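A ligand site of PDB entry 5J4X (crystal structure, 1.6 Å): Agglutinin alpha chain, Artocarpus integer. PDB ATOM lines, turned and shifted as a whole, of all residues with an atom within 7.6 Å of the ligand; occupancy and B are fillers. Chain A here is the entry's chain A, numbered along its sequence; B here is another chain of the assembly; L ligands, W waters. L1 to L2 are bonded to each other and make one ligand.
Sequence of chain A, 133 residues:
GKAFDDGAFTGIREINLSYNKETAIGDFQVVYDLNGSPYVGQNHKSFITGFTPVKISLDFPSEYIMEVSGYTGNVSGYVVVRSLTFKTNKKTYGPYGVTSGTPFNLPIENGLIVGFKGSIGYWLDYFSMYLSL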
ATOM      1  N   GLY A   1       6.956 -19.080  20.961  1.00  0.00           N
ATOM      2  CA  GLY A   1       7.575 -20.472  21.022  1.00  0.00           C
ATOM      3  C   GLY A   1       8.574 -20.583  22.145  1.00  0.00           C
ATOM      4  O   GLY A   1       8.974 -19.574  22.718  1.00  0.00           O
ATOM      5  N   LYS A   2       9.002 -21.802  22.469  1.00  0.00           N
ATOM      6  CA  LYS A   2      10.118 -21.979  23.407  1.00  0.00           C
ATOM      7  C   LYS A   2      11.480 -22.172  22.681  1.00  0.00           C
ATOM      8  O   LYS A   2      11.560 -23.062  21.850  1.00  0.00           O
ATOM      9  CB  LYS A   2       9.915 -23.179  24.301  1.00  0.00           C
ATOM     10  CG  LYS A   2      11.121 -23.383  25.180  1.00  0.00           C
ATOM     11  CD  LYS A   2      11.163 -24.791  25.699  1.00  0.00           C
ATOM     12  CE  LYS A   2      11.925 -24.852  27.024  1.00  0.00           C
ATOM     13  NZ  LYS A   2      11.753 -26.190  27.684  1.00  0.00           N
ATOM     14  N   ILE A  25       5.599 -28.330  10.826  1.00  0.00           N
ATOM     15  CA  ILE A  25       6.539 -29.162  11.597  1.00  0.00           C
ATOM     16  C   ILE A  25       6.286 -28.983  13.094  1.00  0.00           C
ATOM     17  O   ILE A  25       5.931 -27.885  13.528  1.00  0.00           O
ATOM     18  CB  ILE A  25       8.009 -28.831  11.217  1.00  0.00           C
ATOM     19  CG1 ILE A  25       8.332 -29.076   9.708  1.00  0.00           C
ATOM     20  CG2 ILE A  25       8.978 -29.613  12.145  1.00  0.00           C
ATOM     21  CD1 ILE A  25       8.231 -30.490   9.133  1.00  0.00           C
ATOM     22  N   SER A  46       6.804 -29.701  20.378  1.00  0.00           N
ATOM     23  CA  SER A  46       5.567 -28.898  20.220  1.00  0.00           C
ATOM     24  C   SER A  46       4.765 -28.845  21.519  1.00  0.00           C
ATOM     25  O   SER A  46       4.668 -29.854  22.203  1.00  0.00           O
ATOM     26  CB  SER A  46       4.701 -29.545  19.119  1.00  0.00           C
ATOM     27  OG  SER A  46       3.443 -28.867  18.959  1.00  0.00           O
ATOM     28  N   PHE A  47       4.161 -27.697  21.849  1.00  0.00           N
ATOM     29  CA  PHE A  47       3.122 -27.590  22.885  1.00  0.00           C
ATOM     30  C   PHE A  47       1.828 -28.402  22.586  1.00  0.00           C
ATOM     31  O   PHE A  47       0.974 -28.508  23.491  1.00  0.00           O
ATOM     32  CB  PHE A  47       2.640 -26.137  23.097  1.00  0.00           C
ATOM     33  CG  PHE A  47       3.706 -25.126  23.409  1.00  0.00           C
ATOM     34  CD1 PHE A  47       4.977 -25.496  23.775  1.00  0.00           C
ATOM     35  CD2 PHE A  47       3.390 -23.732  23.365  1.00  0.00           C
ATOM     36  CE1 PHE A  47       5.951 -24.527  24.071  1.00  0.00           C
ATOM     37  CE2 PHE A  47       4.357 -22.762  23.650  1.00  0.00           C
ATOM     38  CZ  PHE A  47       5.629 -23.174  24.011  1.00  0.00           C
ATOM     39  N   ILE A  48       1.647 -28.875  21.346  1.00  0.00           N
ATOM     40  CA  ILE A  48       0.441 -29.644  20.952  1.00  0.00           C
ATOM     41  C   ILE A  48       0.764 -31.087  20.506  1.00  0.00           C
ATOM     42  O   ILE A  48       1.909 -31.348  20.168  1.00  0.00           O
ATOM     43  CB  ILE A  48      -0.493 -28.884  19.909  1.00  0.00           C
ATOM     44  CG1 ILE A  48       0.196 -28.611  18.551  1.00  0.00           C
ATOM     45  CG2 ILE A  48      -0.961 -27.558  20.460  1.00  0.00           C
ATOM     46  CD1 ILE A  48      -0.823 -28.282  17.485  1.00  0.00           C
ATOM     47  N   ASN A  74       2.078 -18.792   7.173  1.00  0.00           N
ATOM     48  CA  ASN A  74       1.091 -18.616   8.221  1.00  0.00           C
ATOM     49  C   ASN A  74       0.366 -19.935   8.565  1.00  0.00           C
ATOM     50  O   ASN A  74      -0.071 -20.692   7.645  1.00  0.00           O
ATOM     51  CB  ASN A  74       0.039 -17.514   7.804  1.00  0.00           C
ATOM     52  CG  ASN A  74       0.499 -16.065   8.149  1.00  0.00           C
ATOM     53  OD1 ASN A  74       1.504 -15.876   8.871  1.00  0.00           O
ATOM     54  ND2 ASN A  74      -0.254 -15.032   7.652  1.00  0.00           N
ATOM     55  N   VAL A  75       0.290 -20.235   9.864  1.00  0.00           N
ATOM     56  CA  VAL A  75      -0.655 -21.244  10.373  1.00  0.00           C
ATOM     57  C   VAL A  75      -1.262 -20.655  11.606  1.00  0.00           C
ATOM     58  O   VAL A  75      -0.545 -20.248  12.491  1.00  0.00           O
ATOM     59  CB  VAL A  75       0.049 -22.539  10.808  1.00  0.00           C
ATOM     60  CG1 VAL A  75      -0.981 -23.521  11.363  1.00  0.00           C
ATOM     61  CG2 VAL A  75       0.804 -23.150   9.642  1.00  0.00           C
ATOM     62  N   SER A  76      -2.589 -20.637  11.691  1.00  0.00           N
ATOM     63  CA  SER A  76      -3.267 -19.931  12.801  1.00  0.00           C
ATOM     64  C   SER A  76      -2.724 -18.491  12.989  1.00  0.00           C
ATOM     65  O   SER A  76      -2.701 -17.972  14.094  1.00  0.00           O
ATOM     66  CB  SER A  76      -3.166 -20.755  14.089  1.00  0.00           C
ATOM     67  OG  SER A  76      -3.885 -21.978  13.974  1.00  0.00           O
ATOM     68  N   GLY A  77      -2.279 -17.847  11.913  1.00  0.00           N
ATOM     69  CA  GLY A  77      -1.770 -16.491  12.067  1.00  0.00           C
ATOM     70  C   GLY A  77      -0.299 -16.326  12.416  1.00  0.00           C
ATOM     71  O   GLY A  77       0.223 -15.187  12.379  1.00  0.00           O
ATOM     72  N   TYR A  78       0.390 -17.429  12.719  1.00  0.00           N
ATOM     73  CA  TYR A  78       1.829 -17.377  12.951  1.00  0.00           C
ATOM     74  C   TYR A  78       2.601 -17.867  11.747  1.00  0.00           C
ATOM     75  O   TYR A  78       2.227 -18.897  11.109  1.00  0.00           O
ATOM     76  CB  TYR A  78       2.277 -18.217  14.147  1.00  0.00           C
ATOM     77  CG  TYR A  78       1.456 -18.069  15.378  1.00  0.00           C
ATOM     78  CD1 TYR A  78       1.797 -17.127  16.347  1.00  0.00           C
ATOM     79  CD2 TYR A  78       0.336 -18.915  15.615  1.00  0.00           C
ATOM     80  CE1 TYR A  78       1.047 -16.982  17.501  1.00  0.00           C
ATOM     81  CE2 TYR A  78      -0.402 -18.789  16.768  1.00  0.00           C
ATOM     82  CZ  TYR A  78      -0.040 -17.814  17.698  1.00  0.00           C
ATOM     83  OH  TYR A  78      -0.745 -17.679  18.880  1.00  0.00           O
ATOM     84  N   VAL A  79       3.672 -17.132  11.432  1.00  0.00           N
ATOM     85  CA  VAL A  79       4.670 -17.617  10.484  1.00  0.00           C
ATOM     86  C   VAL A  79       5.391 -18.803  11.106  1.00  0.00           C
ATOM     87  O   VAL A  79       5.999 -18.639  12.165  1.00  0.00           O
ATOM     88  CB  VAL A  79       5.723 -16.520  10.157  1.00  0.00           C
ATOM     89  CG1 VAL A  79       6.694 -16.992   9.071  1.00  0.00           C
ATOM     90  CG2 VAL A  79       5.004 -15.217   9.777  1.00  0.00           C
ATOM     91  N   VAL A  80       5.408 -19.964  10.439  1.00  0.00           N
ATOM     92  CA  VAL A  80       6.041 -21.146  11.030  1.00  0.00           C
ATOM     93  C   VAL A  80       6.735 -21.889   9.906  1.00  0.00           C
ATOM     94  O   VAL A  80       6.502 -21.607   8.750  1.00  0.00           O
ATOM     95  CB  VAL A  80       4.980 -22.008  11.782  1.00  0.00           C
ATOM     96  CG1 VAL A  80       4.367 -21.187  12.923  1.00  0.00           C
ATOM     97  CG2 VAL A  80       3.863 -22.516  10.872  1.00  0.00           C
ATOM     98  N   VAL A  81       7.646 -22.766  10.240  1.00  0.00           N
ATOM     99  CA  VAL A  81       8.214 -23.669   9.238  1.00  0.00           C
ATOM    100  C   VAL A  81       7.213 -24.751   8.875  1.00  0.00           C
ATOM    101  O   VAL A  81       7.065 -25.795   9.584  1.00  0.00           O
ATOM    102  CB  VAL A  81       9.531 -24.311   9.717  1.00  0.00           C
ATOM    103  CG1 VAL A  81      10.113 -25.210   8.644  1.00  0.00           C
ATOM    104  CG2 VAL A  81      10.547 -23.277  10.206  1.00  0.00           C
ATOM    105  N   SER A 119      13.205 -22.371  17.633  1.00  0.00           N
ATOM    106  CA  SER A 119      12.091 -22.181  18.546  1.00  0.00           C
ATOM    107  C   SER A 119      10.859 -22.913  18.069  1.00  0.00           C
ATOM    108  O   SER A 119      10.551 -22.896  16.886  1.00  0.00           O
ATOM    109  CB  SER A 119      11.783 -20.700  18.687  1.00  0.00           C
ATOM    110  OG  SER A 119      10.603 -20.550  19.426  1.00  0.00           O
ATOM    111  N   ILE A 120      10.239 -23.643  19.002  1.00  0.00           N
ATOM    112  CA  ILE A 120       9.019 -24.445  18.782  1.00  0.00           C
ATOM    113  C   ILE A 120       7.962 -23.976  19.807  1.00  0.00           C
ATOM    114  O   ILE A 120       8.232 -23.867  21.044  1.00  0.00           O
ATOM    115  CB  ILE A 120       9.337 -25.949  18.894  1.00  0.00           C
ATOM    116  CG1 ILE A 120      10.435 -26.300  17.928  1.00  0.00           C
ATOM    117  CG2 ILE A 120       8.109 -26.843  18.621  1.00  0.00           C
ATOM    118  CD1 ILE A 120      10.849 -27.756  17.949  1.00  0.00           C
ATOM    119  N   GLY A 121       6.783 -23.616  19.296  1.00  0.00           N
ATOM    120  CA  GLY A 121       5.597 -23.424  20.138  1.00  0.00           C
ATOM    121  C   GLY A 121       4.619 -24.515  19.731  1.00  0.00           C
ATOM    122  O   GLY A 121       4.839 -25.717  20.024  1.00  0.00           O
ATOM    123  N   TYR A 122       3.565 -24.129  19.026  1.00  0.00           N
ATOM    124  CA  TYR A 122       2.642 -25.133  18.507  1.00  0.00           C
ATOM    125  C   TYR A 122       3.323 -25.805  17.311  1.00  0.00           C
ATOM    126  O   TYR A 122       3.174 -26.986  17.137  1.00  0.00           O
ATOM    127  CB  TYR A 122       1.349 -24.522  18.080  1.00  0.00           C
ATOM    128  CG  TYR A 122       0.324 -24.208  19.165  1.00  0.00           C
ATOM    129  CD1 TYR A 122       0.693 -23.767  20.452  1.00  0.00           C
ATOM    130  CD2 TYR A 122      -1.039 -24.269  18.850  1.00  0.00           C
ATOM    131  CE1 TYR A 122      -0.281 -23.441  21.397  1.00  0.00           C
ATOM    132  CE2 TYR A 122      -1.997 -23.980  19.781  1.00  0.00           C
ATOM    133  CZ  TYR A 122      -1.609 -23.523  21.029  1.00  0.00           C
ATOM    134  OH  TYR A 122      -2.621 -23.246  21.928  1.00  0.00           O
ATOM    135  N   TRP A 123       4.085 -25.021  16.524  1.00  0.00           N
ATOM    136  CA  TRP A 123       4.904 -25.487  15.409  1.00  0.00           C
ATOM    137  C   TRP A 123       6.302 -24.932  15.535  1.00  0.00           C
ATOM    138  O   TRP A 123       6.563 -23.958  16.320  1.00  0.00           O
ATOM    139  CB  TRP A 123       4.266 -25.068  14.067  1.00  0.00           C
ATOM    140  CG  TRP A 123       2.834 -25.573  14.039  1.00  0.00           C
ATOM    141  CD1 TRP A 123       2.408 -26.892  13.811  1.00  0.00           C
ATOM    142  CD2 TRP A 123       1.604 -24.833  14.414  1.00  0.00           C
ATOM    143  NE1 TRP A 123       1.037 -26.991  13.936  1.00  0.00           N
ATOM    144  CE2 TRP A 123       0.505 -25.810  14.312  1.00  0.00           C
ATOM    145  CE3 TRP A 123       1.292 -23.479  14.723  1.00  0.00           C
ATOM    146  CZ2 TRP A 123      -0.833 -25.442  14.535  1.00  0.00           C
ATOM    147  CZ3 TRP A 123      -0.054 -23.132  14.968  1.00  0.00           C
ATOM    148  CH2 TRP A 123      -1.078 -24.095  14.874  1.00  0.00           C
ATOM    149  N   LEU A 124       7.228 -25.554  14.786  1.00  0.00           N
ATOM    150  CA  LEU A 124       8.553 -24.991  14.624  1.00  0.00           C
ATOM    151  C   LEU A 124       8.445 -23.535  14.042  1.00  0.00           C
ATOM    152  O   LEU A 124       7.989 -23.333  12.884  1.00  0.00           O
ATOM    153  CB  LEU A 124       9.413 -25.937  13.793  1.00  0.00           C
ATOM    154  CG  LEU A 124      10.781 -25.456  13.375  1.00  0.00           C
ATOM    155  CD1 LEU A 124      11.670 -25.223  14.586  1.00  0.00           C
ATOM    156  CD2 LEU A 124      11.411 -26.476  12.400  1.00  0.00           C
ATOM    157  N   ASP A 125       8.777 -22.552  14.881  1.00  0.00           N
ATOM    158  CA  ASP A 125       8.621 -21.125  14.551  1.00  0.00           C
ATOM    159  C   ASP A 125       9.696 -20.701  13.572  1.00  0.00           C
ATOM    160  O   ASP A 125       9.417 -20.041  12.539  1.00  0.00           O
ATOM    161  CB  ASP A 125       8.741 -20.267  15.821  1.00  0.00           C
ATOM    162  CG  ASP A 125       7.641 -20.590  16.860  1.00  0.00           C
ATOM    163  OD1 ASP A 125       6.439 -20.627  16.484  1.00  0.00           O
ATOM    164  OD2 ASP A 125       8.000 -20.793  18.045  1.00  0.00           O
ATOM    165  N   TYR A 126      10.925 -21.079  13.897  1.00  0.00           N
ATOM    166  CA  TYR A 126      12.066 -20.737  13.092  1.00  0.00           C
ATOM    167  C   TYR A 126      13.228 -21.595  13.482  1.00  0.00           C
ATOM    168  O   TYR A 126      13.218 -22.274  14.582  1.00  0.00           O
ATOM    169  CB  TYR A 126      12.458 -19.275  13.312  1.00  0.00           C
ATOM    170  CG  TYR A 126      12.790 -18.841  14.730  1.00  0.00           C
ATOM    171  CD1 TYR A 126      14.046 -19.092  15.316  1.00  0.00           C
ATOM    172  CD2 TYR A 126      11.853 -18.119  15.477  1.00  0.00           C
ATOM    173  CE1 TYR A 126      14.322 -18.618  16.629  1.00  0.00           C
ATOM    174  CE2 TYR A 126      12.130 -17.662  16.753  1.00  0.00           C
ATOM    175  CZ  TYR A 126      13.349 -17.933  17.338  1.00  0.00           C
ATOM    176  OH  TYR A 126      13.582 -17.489  18.619  1.00  0.00           O
ATOM    177  N   GLY B  15      12.003 -18.743   8.877  1.00  0.00           N
ATOM    178  CA  GLY B  15      10.759 -18.760   9.659  1.00  0.00           C
ATOM    179  C   GLY B  15      10.258 -17.448  10.250  1.00  0.00           C
ATOM    180  O   GLY B  15      10.544 -16.378   9.739  1.00  0.00           O
ATOM    181  N   ALA B  16       9.431 -17.521  11.312  1.00  0.00           N
ATOM    182  CA  ALA B  16       9.022 -16.300  11.995  1.00  0.00           C
ATOM    183  C   ALA B  16      10.241 -15.388  12.294  1.00  0.00           C
ATOM    184  O   ALA B  16      11.227 -15.825  12.878  1.00  0.00           O
ATOM    185  CB  ALA B  16       8.308 -16.612  13.290  1.00  0.00           C
ATOM    186  N   LYS B  17      10.099 -14.113  11.916  1.00  0.00           N
ATOM    187  CA  LYS B  17      11.133 -13.105  12.128  1.00  0.00           C
ATOM    188  C   LYS B  17      10.950 -12.411  13.474  1.00  0.00           C
ATOM    189  O   LYS B  17      11.696 -12.745  14.395  1.00  0.00           O
ATOM    190  CB  LYS B  17      11.172 -12.103  10.962  1.00  0.00           C
HETATM  191  C1  LIG L   1       1.864 -20.385  19.600  1.00  0.00           C
HETATM  192  C2  LIG L   1       2.866 -19.627  20.384  1.00  0.00           C
HETATM  193  C3  LIG L   1       3.506 -18.615  19.344  1.00  0.00           C
HETATM  194  C4  LIG L   1       4.206 -19.463  18.181  1.00  0.00           C
HETATM  195  C5  LIG L   1       3.079 -20.370  17.590  1.00  0.00           C
HETATM  196  C6  LIG L   1       3.429 -21.145  16.353  1.00  0.00           C
HETATM  197  C7  LIG L   1      -0.571 -20.912  19.988  1.00  0.00           C
HETATM  198  O1  LIG L   1       0.845 -20.920  20.547  1.00  0.00           O
HETATM  199  O2  LIG L   1       2.131 -18.937  21.446  1.00  0.00           O
HETATM  200  O3  LIG L   1       4.564 -17.904  20.031  1.00  0.00           O
HETATM  201  O4  LIG L   1       5.275 -20.141  18.862  1.00  0.00           O
HETATM  202  O5  LIG L   1       2.587 -21.247  18.673  1.00  0.00           O
HETATM  203  O6  LIG L   1       4.260 -22.228  16.826  1.00  0.00           O
HETATM  204  C1  LG2 L   2       4.629 -16.612  19.427  1.00  0.00           C
HETATM  205  C2  LG2 L   2       5.331 -15.541  20.355  1.00  0.00           C
HETATM  206  C3  LG2 L   2       5.450 -14.187  19.585  1.00  0.00           C
HETATM  207  C4  LG2 L   2       6.238 -14.569  18.298  1.00  0.00           C
HETATM  208  C5  LG2 L   2       5.430 -15.622  17.422  1.00  0.00           C
HETATM  209  C6  LG2 L   2       6.160 -15.928  16.104  1.00  0.00           C
HETATM  210  O1  LG2 L   2       4.476 -15.414  21.487  1.00  0.00           O
HETATM  211  O2  LG2 L   2       6.303 -13.284  20.365  1.00  0.00           O
HETATM  212  O3  LG2 L   2       7.550 -15.170  18.818  1.00  0.00           O
HETATM  213  O4  LG2 L   2       5.379 -16.850  18.231  1.00  0.00           O
HETATM  214  O5  LG2 L   2       5.319 -15.597  14.962  1.00  0.00           O
HETATM  215  O   HOH W   1       1.830 -14.960  21.621  1.00  0.00           O
HETATM  216  O   HOH W   2       5.621 -12.768  23.009  1.00  0.00           O
HETATM  217  O   HOH W   3       5.739 -18.392  14.607  1.00  0.00           O
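O4 of LIG L1 is in hydrogen-bond range of OD1 of Asp 125 (2.7 Å). O of Trp 123 lies within hydrogen-bond range of O6 of LIG L1, at 2.9 Å. The backbone NH (N) of Tyr 122 sits at hydrogen-bond distance from an oxygen (O6) of LIG L1, at 3.0 Å. N of Gly 1 sits at hydrogen-bond distance from O3 of LIG L1 (2.8 Å). O6 of LIG L1 sits at hydrogen-bond distance from N of Trp 123 (2.8 Å).
OH of Tyr 78 touches C7 of LIG L1, 3.4 Å away. Val 80 touches the ligand. Gly 121 touches the ligand. CB of Ala 16 of chain B touches O5 of LG2 L2 (3.6 Å). Hydrophobic or aromatic side chains within 4 Å of the ligand: Tyr 78, Val 80, Tyr 122, Trp 123 and Ala 16 of chain B. Of the 25 residues printed, 8 come within 4 Å of the ligand. Along chain A the residues within 4 Å of the ligand span positions 1 to 125. The nearest printed residue that does not touch the ligand is Val 79 (4.2 Å).
The backbone carbonyl oxygen of Ser 119 sits at hydrogen-bond distance from the backbone NH of Asp 125, 2.7 Å away. The backbone NH (N) of Phe 47 sits at hydrogen-bond distance from the backbone carbonyl oxygen (O) of Gly 121 (2.8 Å). The side-chain hydroxyl of Ser 46 lies within hydrogen-bond range of the backbone carbonyl oxygen of Tyr 122, 2.6 Å away. OD2 of Asp 125 sits at hydrogen-bond distance from N of Gly 121 (3.3 Å). The backbone carbonyl oxygen (O) of Asp 125 sits at hydrogen-bond distance from the backbone NH (N) of Ala 16 of chain B (2.8 Å).
Water W3 lies within hydrogen-bond range of the backbone carbonyl oxygen (O) of Val 79, an oxygen (O5) of LG2 L2 and the side-chain carboxylate (OD1) of Asp 125.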
